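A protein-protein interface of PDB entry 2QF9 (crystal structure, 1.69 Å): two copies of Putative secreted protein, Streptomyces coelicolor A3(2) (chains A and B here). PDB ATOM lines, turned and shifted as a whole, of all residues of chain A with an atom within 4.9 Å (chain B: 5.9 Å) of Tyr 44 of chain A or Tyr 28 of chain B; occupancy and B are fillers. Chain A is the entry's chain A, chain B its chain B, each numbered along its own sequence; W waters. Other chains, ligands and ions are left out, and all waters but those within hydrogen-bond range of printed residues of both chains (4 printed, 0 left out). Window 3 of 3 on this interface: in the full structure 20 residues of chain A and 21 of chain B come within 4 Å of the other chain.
Among the printed residues, pairs that only touch across the chains: Tyr 28 of chain A with Tyr 28 of chain B (3.7 Å), Tyr 28 of chain A with Arg 31 of chain B (3.6 Å), Tyr 28 of chain A with Ala 47 of chain B (3.4 Å), Arg 31 of chain A with Tyr 28 of chain B (3.7 Å), Tyr 44 of chain A with Tyr 28 of chain B (3.5 Å), Ala 47 of chain A with Tyr 28 of chain B (3.4 Å), Gln 48 of chain A with Val 24 of chain B (3.5 Å) and Gln 48 of chain A with Tyr 28 of chain B (3.8 Å).
OD1 of Asp 32 of chain B is in salt-bridge range of NH2 of Arg 31 of chain A (3.8 Å). The guanidinium group of Arg 40 of chain A lies within salt-bridge range of the side-chain carboxylate of Asp 32 of chain B (3.0 Å). The side-chain carboxylate of Glu 25 of chain B is in hydrogen-bond range of the side-chain hydroxyl of Tyr 44 of chain A (2.5 Å). OE1 of Gln 48 of chain A lies within hydrogen-bond range of NE2 of Gln 21 of chain B.
The guanidinium group (NH1) of Arg 40 of chain A is in hydrogen-bond range of the backbone carbonyl oxygen (O) of Arg 31 of chain A.
Of the 14 printed residues of chain B, 7 touch a printed residue of chain A. Hydrophobic or aromatic side chains of chain B that line the printed part of chain A: Val 24, Tyr 28 and Ala 47. Of the 12 printed residues of chain A, 6 touch a printed residue of chain B. Among the printed residues, Asp or Glu carboxylates within 4 Å of a Lys or Arg side-chain nitrogen of the other chain: Arg 31 of chain A with Asp 32 of chain B and Arg 40 of chain A with Asp 32 of chain B.
Tyr 28 of chain B touches its own counterpart, Tyr 28 of chain A. Tyr 28 of chain A touches Arg 31 of chain B, and with the chains exchanged Arg 31 of chain A touches Tyr 28 of chain B. Tyr 28 of chain A touches Ala 47 of chain B, and with the chains exchanged Ala 47 of chain A touches Tyr 28 of chain B. 4 positions are printed for both chains.
Water W3 bridges the side-chain hydroxyl of Tyr 44 of chain A (2.5 Å) and the side-chain carboxylate of Glu 25 of chain B (3.3 Å). Water W2 lies within hydrogen-bond range of O of Tyr 28 of chain A (2.7 Å) and NH2 of Arg 31 of chain B (3.0 Å). Water W4 lies within hydrogen-bond range of O of Tyr 28 of chain B (2.8 Å), NH2 of Arg 31 of chain A (3.0 Å) and OD1 of Asp 32 of chain B (3.2 Å). Water W1 bridges the guanidinium group of Arg 40 of chain A and the side-chain carboxylate of Asp 32 of chain B.
Tyr 44 of chain A touches just these residues of chain B: Glu 25 (2.5 Å) and Tyr 28 (3.5 Å). Tyr 28 of chain B touches just these residues of chain A: Tyr 28, Arg 31, Tyr 44, Ala 47 and Gln 48. Of the printed residues of chain B, Gln 48 of chain A touches Gln 21 (3.0 Å), Val 24 (3.5 Å) and Tyr 28 (3.8 Å). Printed residues of chain B within 4 Å of Arg 31 of chain A: Tyr 28 (3.7 Å) and Asp 32 (3.8 Å). Printed residues of chain A within 4 Å of Gln 21 of chain B: Gln 48 (3.0 Å). Leu 42 of chain A touches none of the printed residues of chain B. Ala 43 of chain B touches none of the printed residues of chain A. The nearest residue of chain B that does not touch Tyr 44 of chain A is Gln 21 of chain B (4.8 Å). The nearest printed residue of chain A that does not touch Tyr 28 of chain B is Ala 43 of chain A (5.5 Å). The nearest printed residue of chain B that does not touch Arg 40 of chain A is Tyr 28 of chain B (6.5 Å).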
ATOM      1  N   TYR A  28     -13.527 -26.914  -7.683  1.00  0.00           N
ATOM      2  CA  TYR A  28     -14.818 -26.728  -8.338  1.00  0.00           C
ATOM      3  C   TYR A  28     -15.893 -27.603  -7.698  1.00  0.00           C
ATOM      4  O   TYR A  28     -17.011 -27.145  -7.479  1.00  0.00           O
ATOM      5  CB  TYR A  28     -14.734 -27.040  -9.841  1.00  0.00           C
ATOM      6  CG  TYR A  28     -14.402 -25.803 -10.637  1.00  0.00           C
ATOM      7  CD1 TYR A  28     -13.073 -25.498 -10.983  1.00  0.00           C
ATOM      8  CD2 TYR A  28     -15.411 -24.893 -10.987  1.00  0.00           C
ATOM      9  CE1 TYR A  28     -12.770 -24.328 -11.702  1.00  0.00           C
ATOM     10  CE2 TYR A  28     -15.106 -23.708 -11.721  1.00  0.00           C
ATOM     11  CZ  TYR A  28     -13.792 -23.438 -12.048  1.00  0.00           C
ATOM     12  OH  TYR A  28     -13.489 -22.290 -12.754  1.00  0.00           O
ATOM     13  N   ARG A  31     -16.946 -26.478  -4.014  1.00  0.00           N
ATOM     14  CA  ARG A  31     -17.664 -25.213  -3.973  1.00  0.00           C
ATOM     15  C   ARG A  31     -19.142 -25.399  -4.314  1.00  0.00           C
ATOM     16  O   ARG A  31     -19.992 -24.613  -3.870  1.00  0.00           O
ATOM     17  CB  ARG A  31     -16.987 -24.148  -4.841  1.00  0.00           C
ATOM     18  CG  ARG A  31     -15.716 -23.580  -4.189  1.00  0.00           C
ATOM     19  CD  ARG A  31     -14.969 -22.641  -5.158  1.00  0.00           C
ATOM     20  NE  ARG A  31     -15.853 -21.645  -5.775  1.00  0.00           N
ATOM     21  CZ  ARG A  31     -16.184 -20.477  -5.230  1.00  0.00           C
ATOM     22  NH1 ARG A  31     -15.733 -20.140  -4.029  1.00  0.00           N
ATOM     23  NH2 ARG A  31     -16.988 -19.647  -5.881  1.00  0.00           N
ATOM     24  N   VAL A  39     -14.245 -22.577   3.646  1.00  0.00           N
ATOM     25  CA  VAL A  39     -13.827 -23.638   2.707  1.00  0.00           C
ATOM     26  C   VAL A  39     -14.030 -23.194   1.257  1.00  0.00           C
ATOM     27  O   VAL A  39     -13.153 -23.419   0.415  1.00  0.00           O
ATOM     28  CB  VAL A  39     -14.529 -24.987   3.025  1.00  0.00           C
ATOM     29  CG1 VAL A  39     -14.284 -26.022   1.921  1.00  0.00           C
ATOM     30  CG2 VAL A  39     -14.030 -25.503   4.376  1.00  0.00           C
ATOM     31  N   ARG A  40     -15.145 -22.525   0.963  1.00  0.00           N
ATOM     32  CA  ARG A  40     -15.329 -21.990  -0.397  1.00  0.00           C
ATOM     33  C   ARG A  40     -14.234 -21.002  -0.789  1.00  0.00           C
ATOM     34  O   ARG A  40     -13.771 -21.034  -1.947  1.00  0.00           O
ATOM     35  CB  ARG A  40     -16.720 -21.364  -0.578  1.00  0.00           C
ATOM     36  CG  ARG A  40     -17.824 -22.418  -0.752  1.00  0.00           C
ATOM     37  CD  ARG A  40     -19.216 -21.813  -0.785  1.00  0.00           C
ATOM     38  NE  ARG A  40     -19.318 -20.576  -1.574  1.00  0.00           N
ATOM     39  CZ  ARG A  40     -19.524 -20.537  -2.890  1.00  0.00           C
ATOM     40  NH1 ARG A  40     -19.655 -21.654  -3.597  1.00  0.00           N
ATOM     41  NH2 ARG A  40     -19.614 -19.378  -3.498  1.00  0.00           N
ATOM     42  N   ARG A  41     -13.806 -20.162   0.165  1.00  0.00           N
ATOM     43  CA  ARG A  41     -12.748 -19.170  -0.107  1.00  0.00           C
ATOM     44  C   ARG A  41     -11.416 -19.879  -0.334  1.00  0.00           C
ATOM     45  O   ARG A  41     -10.678 -19.533  -1.260  1.00  0.00           O
ATOM     46  CB  ARG A  41     -12.613 -18.117   1.002  1.00  0.00           C
ATOM     47  CG  ARG A  41     -11.459 -17.146   0.775  1.00  0.00           C
ATOM     48  CD  ARG A  41     -11.689 -16.260  -0.446  1.00  0.00           C
ATOM     49  NE  ARG A  41     -10.445 -15.708  -0.996  1.00  0.00           N
ATOM     50  CZ  ARG A  41     -10.363 -14.687  -1.855  1.00  0.00           C
ATOM     51  NH1 ARG A  41     -11.456 -14.045  -2.274  1.00  0.00           N
ATOM     52  NH2 ARG A  41      -9.172 -14.297  -2.295  1.00  0.00           N
ATOM     53  N   LEU A  42     -11.107 -20.865   0.515  1.00  0.00           N
ATOM     54  CA  LEU A  42      -9.874 -21.620   0.351  1.00  0.00           C
ATOM     55  C   LEU A  42      -9.854 -22.294  -1.023  1.00  0.00           C
ATOM     56  O   LEU A  42      -8.841 -22.207  -1.758  1.00  0.00           O
ATOM     57  CB  LEU A  42      -9.735 -22.667   1.460  1.00  0.00           C
ATOM     58  CG  LEU A  42      -8.581 -23.671   1.310  1.00  0.00           C
ATOM     59  CD1 LEU A  42      -7.190 -22.969   1.268  1.00  0.00           C
ATOM     60  CD2 LEU A  42      -8.684 -24.749   2.398  1.00  0.00           C
ATOM     61  N   ALA A  43     -10.969 -22.952  -1.369  1.00  0.00           N
ATOM     62  CA  ALA A  43     -11.080 -23.662  -2.652  1.00  0.00           C
ATOM     63  C   ALA A  43     -10.890 -22.690  -3.823  1.00  0.00           C
ATOM     64  O   ALA A  43     -10.203 -22.996  -4.784  1.00  0.00           O
ATOM     65  CB  ALA A  43     -12.422 -24.394  -2.749  1.00  0.00           C
ATOM     66  N   TYR A  44     -11.450 -21.494  -3.705  1.00  0.00           N
ATOM     67  CA  TYR A  44     -11.287 -20.471  -4.746  1.00  0.00           C
ATOM     68  C   TYR A  44      -9.807 -20.072  -4.873  1.00  0.00           C
ATOM     69  O   TYR A  44      -9.272 -20.001  -5.982  1.00  0.00           O
ATOM     70  CB  TYR A  44     -12.164 -19.257  -4.416  1.00  0.00           C
ATOM     71  CG  TYR A  44     -11.928 -18.040  -5.267  1.00  0.00           C
ATOM     72  CD1 TYR A  44     -12.579 -17.883  -6.494  1.00  0.00           C
ATOM     73  CD2 TYR A  44     -11.068 -17.026  -4.837  1.00  0.00           C
ATOM     74  CE1 TYR A  44     -12.368 -16.748  -7.276  1.00  0.00           C
ATOM     75  CE2 TYR A  44     -10.849 -15.888  -5.615  1.00  0.00           C
ATOM     76  CZ  TYR A  44     -11.510 -15.764  -6.827  1.00  0.00           C
ATOM     77  OH  TYR A  44     -11.305 -14.634  -7.599  1.00  0.00           O
ATOM     78  N   ASP A  45      -9.158 -19.805  -3.739  1.00  0.00           N
ATOM     79  CA  ASP A  45      -7.730 -19.447  -3.734  1.00  0.00           C
ATOM     80  C   ASP A  45      -6.818 -20.535  -4.318  1.00  0.00           C
ATOM     81  O   ASP A  45      -5.935 -20.255  -5.129  1.00  0.00           O
ATOM     82  CB  ASP A  45      -7.269 -19.041  -2.336  1.00  0.00           C
ATOM     83  CG  ASP A  45      -7.880 -17.696  -1.884  1.00  0.00           C
ATOM     84  OD1 ASP A  45      -8.298 -16.895  -2.737  1.00  0.00           O
ATOM     85  OD2 ASP A  45      -7.920 -17.437  -0.674  1.00  0.00           O
ATOM     86  N   ILE A  46      -7.058 -21.777  -3.925  1.00  0.00           N
ATOM     87  CA  ILE A  46      -6.306 -22.887  -4.495  1.00  0.00           C
ATOM     88  C   ILE A  46      -6.560 -23.018  -6.001  1.00  0.00           C
ATOM     89  O   ILE A  46      -5.614 -23.216  -6.770  1.00  0.00           O
ATOM     90  CB  ILE A  46      -6.622 -24.210  -3.758  1.00  0.00           C
ATOM     91  CG1 ILE A  46      -6.046 -24.133  -2.342  1.00  0.00           C
ATOM     92  CG2 ILE A  46      -6.057 -25.438  -4.539  1.00  0.00           C
ATOM     93  CD1 ILE A  46      -6.431 -25.321  -1.444  1.00  0.00           C
ATOM     94  N   ALA A  47      -7.832 -22.951  -6.420  1.00  0.00           N
ATOM     95  CA  ALA A  47      -8.145 -23.013  -7.847  1.00  0.00           C
ATOM     96  C   ALA A  47      -7.416 -21.909  -8.628  1.00  0.00           C
ATOM     97  O   ALA A  47      -6.828 -22.160  -9.679  1.00  0.00           O
ATOM     98  CB  ALA A  47      -9.664 -22.915  -8.083  1.00  0.00           C
ATOM     99  N   GLN A  48      -7.471 -20.691  -8.108  1.00  0.00           N
ATOM    100  CA  GLN A  48      -6.868 -19.543  -8.791  1.00  0.00           C
ATOM    101  C   GLN A  48      -5.356 -19.707  -8.923  1.00  0.00           C
ATOM    102  O   GLN A  48      -4.791 -19.513 -10.017  1.00  0.00           O
ATOM    103  CB  GLN A  48      -7.246 -18.236  -8.088  1.00  0.00           C
ATOM    104  CG  GLN A  48      -8.720 -17.847  -8.315  1.00  0.00           C
ATOM    105  CD  GLN A  48      -8.928 -17.200  -9.681  1.00  0.00           C
ATOM    106  OE1 GLN A  48      -8.927 -15.979  -9.795  1.00  0.00           O
ATOM    107  NE2 GLN A  48      -9.072 -18.011 -10.715  1.00  0.00           N
ATOM    108  N   GLN B  21      -8.193 -12.084 -16.462  1.00  0.00           N
ATOM    109  CA  GLN B  21      -8.527 -12.183 -15.021  1.00  0.00           C
ATOM    110  C   GLN B  21      -9.982 -11.750 -14.740  1.00  0.00           C
ATOM    111  O   GLN B  21     -10.699 -12.360 -13.930  1.00  0.00           O
ATOM    112  CB  GLN B  21      -7.562 -11.366 -14.152  1.00  0.00           C
ATOM    113  CG  GLN B  21      -7.704 -11.698 -12.625  1.00  0.00           C
ATOM    114  CD  GLN B  21      -7.871 -13.220 -12.334  1.00  0.00           C
ATOM    115  OE1 GLN B  21      -7.076 -14.060 -12.785  1.00  0.00           O
ATOM    116  NE2 GLN B  21      -8.939 -13.573 -11.593  1.00  0.00           N
ATOM    117  N   ALA B  23     -12.563 -11.857 -16.873  1.00  0.00           N
ATOM    118  CA  ALA B  23     -13.472 -12.871 -17.434  1.00  0.00           C
ATOM    119  C   ALA B  23     -13.598 -14.053 -16.488  1.00  0.00           C
ATOM    120  O   ALA B  23     -14.686 -14.607 -16.309  1.00  0.00           O
ATOM    121  CB  ALA B  23     -12.985 -13.343 -18.777  1.00  0.00           C
ATOM    122  N   VAL B  24     -12.466 -14.460 -15.910  1.00  0.00           N
ATOM    123  CA  VAL B  24     -12.478 -15.541 -14.913  1.00  0.00           C
ATOM    124  C   VAL B  24     -13.366 -15.137 -13.724  1.00  0.00           C
ATOM    125  O   VAL B  24     -14.227 -15.905 -13.308  1.00  0.00           O
ATOM    126  CB  VAL B  24     -11.064 -15.907 -14.444  1.00  0.00           C
ATOM    127  CG1 VAL B  24     -11.136 -16.984 -13.353  1.00  0.00           C
ATOM    128  CG2 VAL B  24     -10.217 -16.405 -15.638  1.00  0.00           C
ATOM    129  N   GLU B  25     -13.173 -13.925 -13.203  1.00  0.00           N
ATOM    130  CA  GLU B  25     -13.994 -13.456 -12.082  1.00  0.00           C
ATOM    131  C   GLU B  25     -15.488 -13.447 -12.443  1.00  0.00           C
ATOM    132  O   GLU B  25     -16.314 -13.905 -11.650  1.00  0.00           O
ATOM    133  CB  GLU B  25     -13.536 -12.078 -11.588  1.00  0.00           C
ATOM    134  CG  GLU B  25     -14.164 -11.674 -10.267  1.00  0.00           C
ATOM    135  CD  GLU B  25     -13.809 -12.668  -9.148  1.00  0.00           C
ATOM    136  OE1 GLU B  25     -12.645 -13.159  -9.120  1.00  0.00           O
ATOM    137  OE2 GLU B  25     -14.700 -12.992  -8.336  1.00  0.00           O
ATOM    138  N   MET B  26     -15.818 -12.950 -13.633  1.00  0.00           N
ATOM    139  CA  MET B  26     -17.206 -12.868 -14.051  1.00  0.00           C
ATOM    140  C   MET B  26     -17.840 -14.261 -14.116  1.00  0.00           C
ATOM    141  O   MET B  26     -19.017 -14.452 -13.777  1.00  0.00           O
ATOM    142  CB  MET B  26     -17.293 -12.196 -15.411  1.00  0.00           C
ATOM    143  CG  MET B  26     -18.659 -11.668 -15.685  1.00  0.00           C
ATOM    144  SD  MET B  26     -18.816 -11.117 -17.495  1.00  0.00           S
ATOM    145  CE  MET B  26     -17.824  -9.443 -17.387  1.00  0.00           C
ATOM    146  N   SER B  27     -17.038 -15.230 -14.537  1.00  0.00           N
ATOM    147  CA  SER B  27     -17.481 -16.623 -14.610  1.00  0.00           C
ATOM    148  C   SER B  27     -17.746 -17.219 -13.217  1.00  0.00           C
ATOM    149  O   SER B  27     -18.753 -17.910 -13.016  1.00  0.00           O
ATOM    150  CB  SER B  27     -16.468 -17.430 -15.429  1.00  0.00           C
ATOM    151  OG  SER B  27     -16.460 -16.922 -16.760  1.00  0.00           O
ATOM    152  N   TYR B  28     -16.884 -16.914 -12.252  1.00  0.00           N
ATOM    153  CA  TYR B  28     -17.115 -17.280 -10.857  1.00  0.00           C
ATOM    154  C   TYR B  28     -18.422 -16.657 -10.345  1.00  0.00           C
ATOM    155  O   TYR B  28     -19.202 -17.316  -9.667  1.00  0.00           O
ATOM    156  CB  TYR B  28     -15.935 -16.867  -9.977  1.00  0.00           C
ATOM    157  CG  TYR B  28     -14.886 -17.968  -9.862  1.00  0.00           C
ATOM    158  CD1 TYR B  28     -13.759 -17.977 -10.681  1.00  0.00           C
ATOM    159  CD2 TYR B  28     -15.057 -19.023  -8.964  1.00  0.00           C
ATOM    160  CE1 TYR B  28     -12.788 -19.001 -10.575  1.00  0.00           C
ATOM    161  CE2 TYR B  28     -14.107 -20.054  -8.846  1.00  0.00           C
ATOM    162  CZ  TYR B  28     -12.975 -20.038  -9.663  1.00  0.00           C
ATOM    163  OH  TYR B  28     -12.039 -21.055  -9.563  1.00  0.00           O
ATOM    164  N   ILE B  29     -18.647 -15.390 -10.670  1.00  0.00           N
ATOM    165  CA  ILE B  29     -19.852 -14.703 -10.202  1.00  0.00           C
ATOM    166  C   ILE B  29     -21.112 -15.390 -10.740  1.00  0.00           C
ATOM    167  O   ILE B  29     -21.994 -15.742  -9.943  1.00  0.00           O
ATOM    168  CB  ILE B  29     -19.856 -13.209 -10.561  1.00  0.00           C
ATOM    169  CG1 ILE B  29     -18.768 -12.466  -9.779  1.00  0.00           C
ATOM    170  CG2 ILE B  29     -21.228 -12.563 -10.257  1.00  0.00           C
ATOM    171  CD1 ILE B  29     -18.419 -11.133 -10.408  1.00  0.00           C
ATOM    172  N   VAL B  30     -21.199 -15.586 -12.060  1.00  0.00           N
ATOM    173  CA  VAL B  30     -22.427 -16.156 -12.636  1.00  0.00           C
ATOM    174  C   VAL B  30     -22.697 -17.558 -12.095  1.00  0.00           C
ATOM    175  O   VAL B  30     -23.852 -17.921 -11.896  1.00  0.00           O
ATOM    176  CB  VAL B  30     -22.480 -16.123 -14.194  1.00  0.00           C
ATOM    177  CG1 VAL B  30     -21.567 -17.188 -14.837  1.00  0.00           C
ATOM    178  CG2 VAL B  30     -23.952 -16.254 -14.690  1.00  0.00           C
ATOM    179  N   ARG B  31     -21.633 -18.335 -11.853  1.00  0.00           N
ATOM    180  CA  ARG B  31     -21.821 -19.705 -11.365  1.00  0.00           C
ATOM    181  C   ARG B  31     -22.459 -19.704  -9.972  1.00  0.00           C
ATOM    182  O   ARG B  31     -23.145 -20.672  -9.618  1.00  0.00           O
ATOM    183  CB  ARG B  31     -20.506 -20.485 -11.400  1.00  0.00           C
ATOM    184  CG  ARG B  31     -20.221 -20.970 -12.823  1.00  0.00           C
ATOM    185  CD  ARG B  31     -18.884 -21.721 -12.968  1.00  0.00           C
ATOM    186  NE  ARG B  31     -18.765 -22.836 -12.026  1.00  0.00           N
ATOM    187  CZ  ARG B  31     -19.208 -24.082 -12.223  1.00  0.00           C
ATOM    188  NH1 ARG B  31     -19.824 -24.443 -13.353  1.00  0.00           N
ATOM    189  NH2 ARG B  31     -19.016 -24.987 -11.265  1.00  0.00           N
ATOM    190  N   ASP B  32     -22.246 -18.608  -9.227  1.00  0.00           N
ATOM    191  CA  ASP B  32     -22.864 -18.397  -7.895  1.00  0.00           C
ATOM    192  C   ASP B  32     -24.304 -17.900  -7.960  1.00  0.00           C
ATOM    193  O   ASP B  32     -25.027 -17.958  -6.946  1.00  0.00           O
ATOM    194  CB  ASP B  32     -22.071 -17.378  -7.066  1.00  0.00           C
ATOM    195  CG  ASP B  32     -20.849 -17.976  -6.385  1.00  0.00           C
ATOM    196  OD1 ASP B  32     -20.769 -19.222  -6.241  1.00  0.00           O
ATOM    197  OD2 ASP B  32     -19.963 -17.171  -5.982  1.00  0.00           O
ATOM    198  N   ARG B  33     -24.712 -17.383  -9.114  1.00  0.00           N
ATOM    199  CA  ARG B  33     -25.991 -16.656  -9.208  1.00  0.00           C
ATOM    200  C   ARG B  33     -27.125 -17.420  -9.901  1.00  0.00           C
ATOM    201  O   ARG B  33     -28.288 -17.020  -9.808  1.00  0.00           O
ATOM    202  CB  ARG B  33     -25.801 -15.298  -9.886  1.00  0.00           C
ATOM    203  CG  ARG B  33     -24.776 -14.350  -9.246  1.00  0.00           C
ATOM    204  CD  ARG B  33     -25.015 -14.135  -7.771  1.00  0.00           C
ATOM    205  NE  ARG B  33     -26.342 -13.573  -7.480  1.00  0.00           N
ATOM    206  CZ  ARG B  33     -26.768 -13.297  -6.251  1.00  0.00           C
ATOM    207  NH1 ARG B  33     -25.968 -13.525  -5.223  1.00  0.00           N
ATOM    208  NH2 ARG B  33     -27.971 -12.778  -6.043  1.00  0.00           N
ATOM    209  N   ALA B  43     -19.578 -20.960 -18.338  1.00  0.00           N
ATOM    210  CA  ALA B  43     -18.747 -20.191 -17.415  1.00  0.00           C
ATOM    211  C   ALA B  43     -17.519 -20.983 -16.953  1.00  0.00           C
ATOM    212  O   ALA B  43     -16.417 -20.442 -16.864  1.00  0.00           O
ATOM    213  CB  ALA B  43     -19.567 -19.746 -16.214  1.00  0.00           C
ATOM    214  N   ALA B  47     -13.727 -19.769 -17.679  1.00  0.00           N
ATOM    215  CA  ALA B  47     -12.830 -19.591 -16.530  1.00  0.00           C
ATOM    216  C   ALA B  47     -11.588 -20.472 -16.719  1.00  0.00           C
ATOM    217  O   ALA B  47     -10.450 -20.021 -16.559  1.00  0.00           O
ATOM    218  CB  ALA B  47     -13.546 -19.945 -15.228  1.00  0.00           C
HETATM  219  O   HOH W   1     -19.470 -16.630  -2.582  1.00  0.00           O
HETATM  220  O   HOH W   2     -18.028 -24.793  -8.440  1.00  0.00           O
HETATM  221  O   HOH W   3      -9.953 -12.577  -7.291  1.00  0.00           O
HETATM  222  O   HOH W   4     -18.512 -19.720  -8.444  1.00  0.00           O
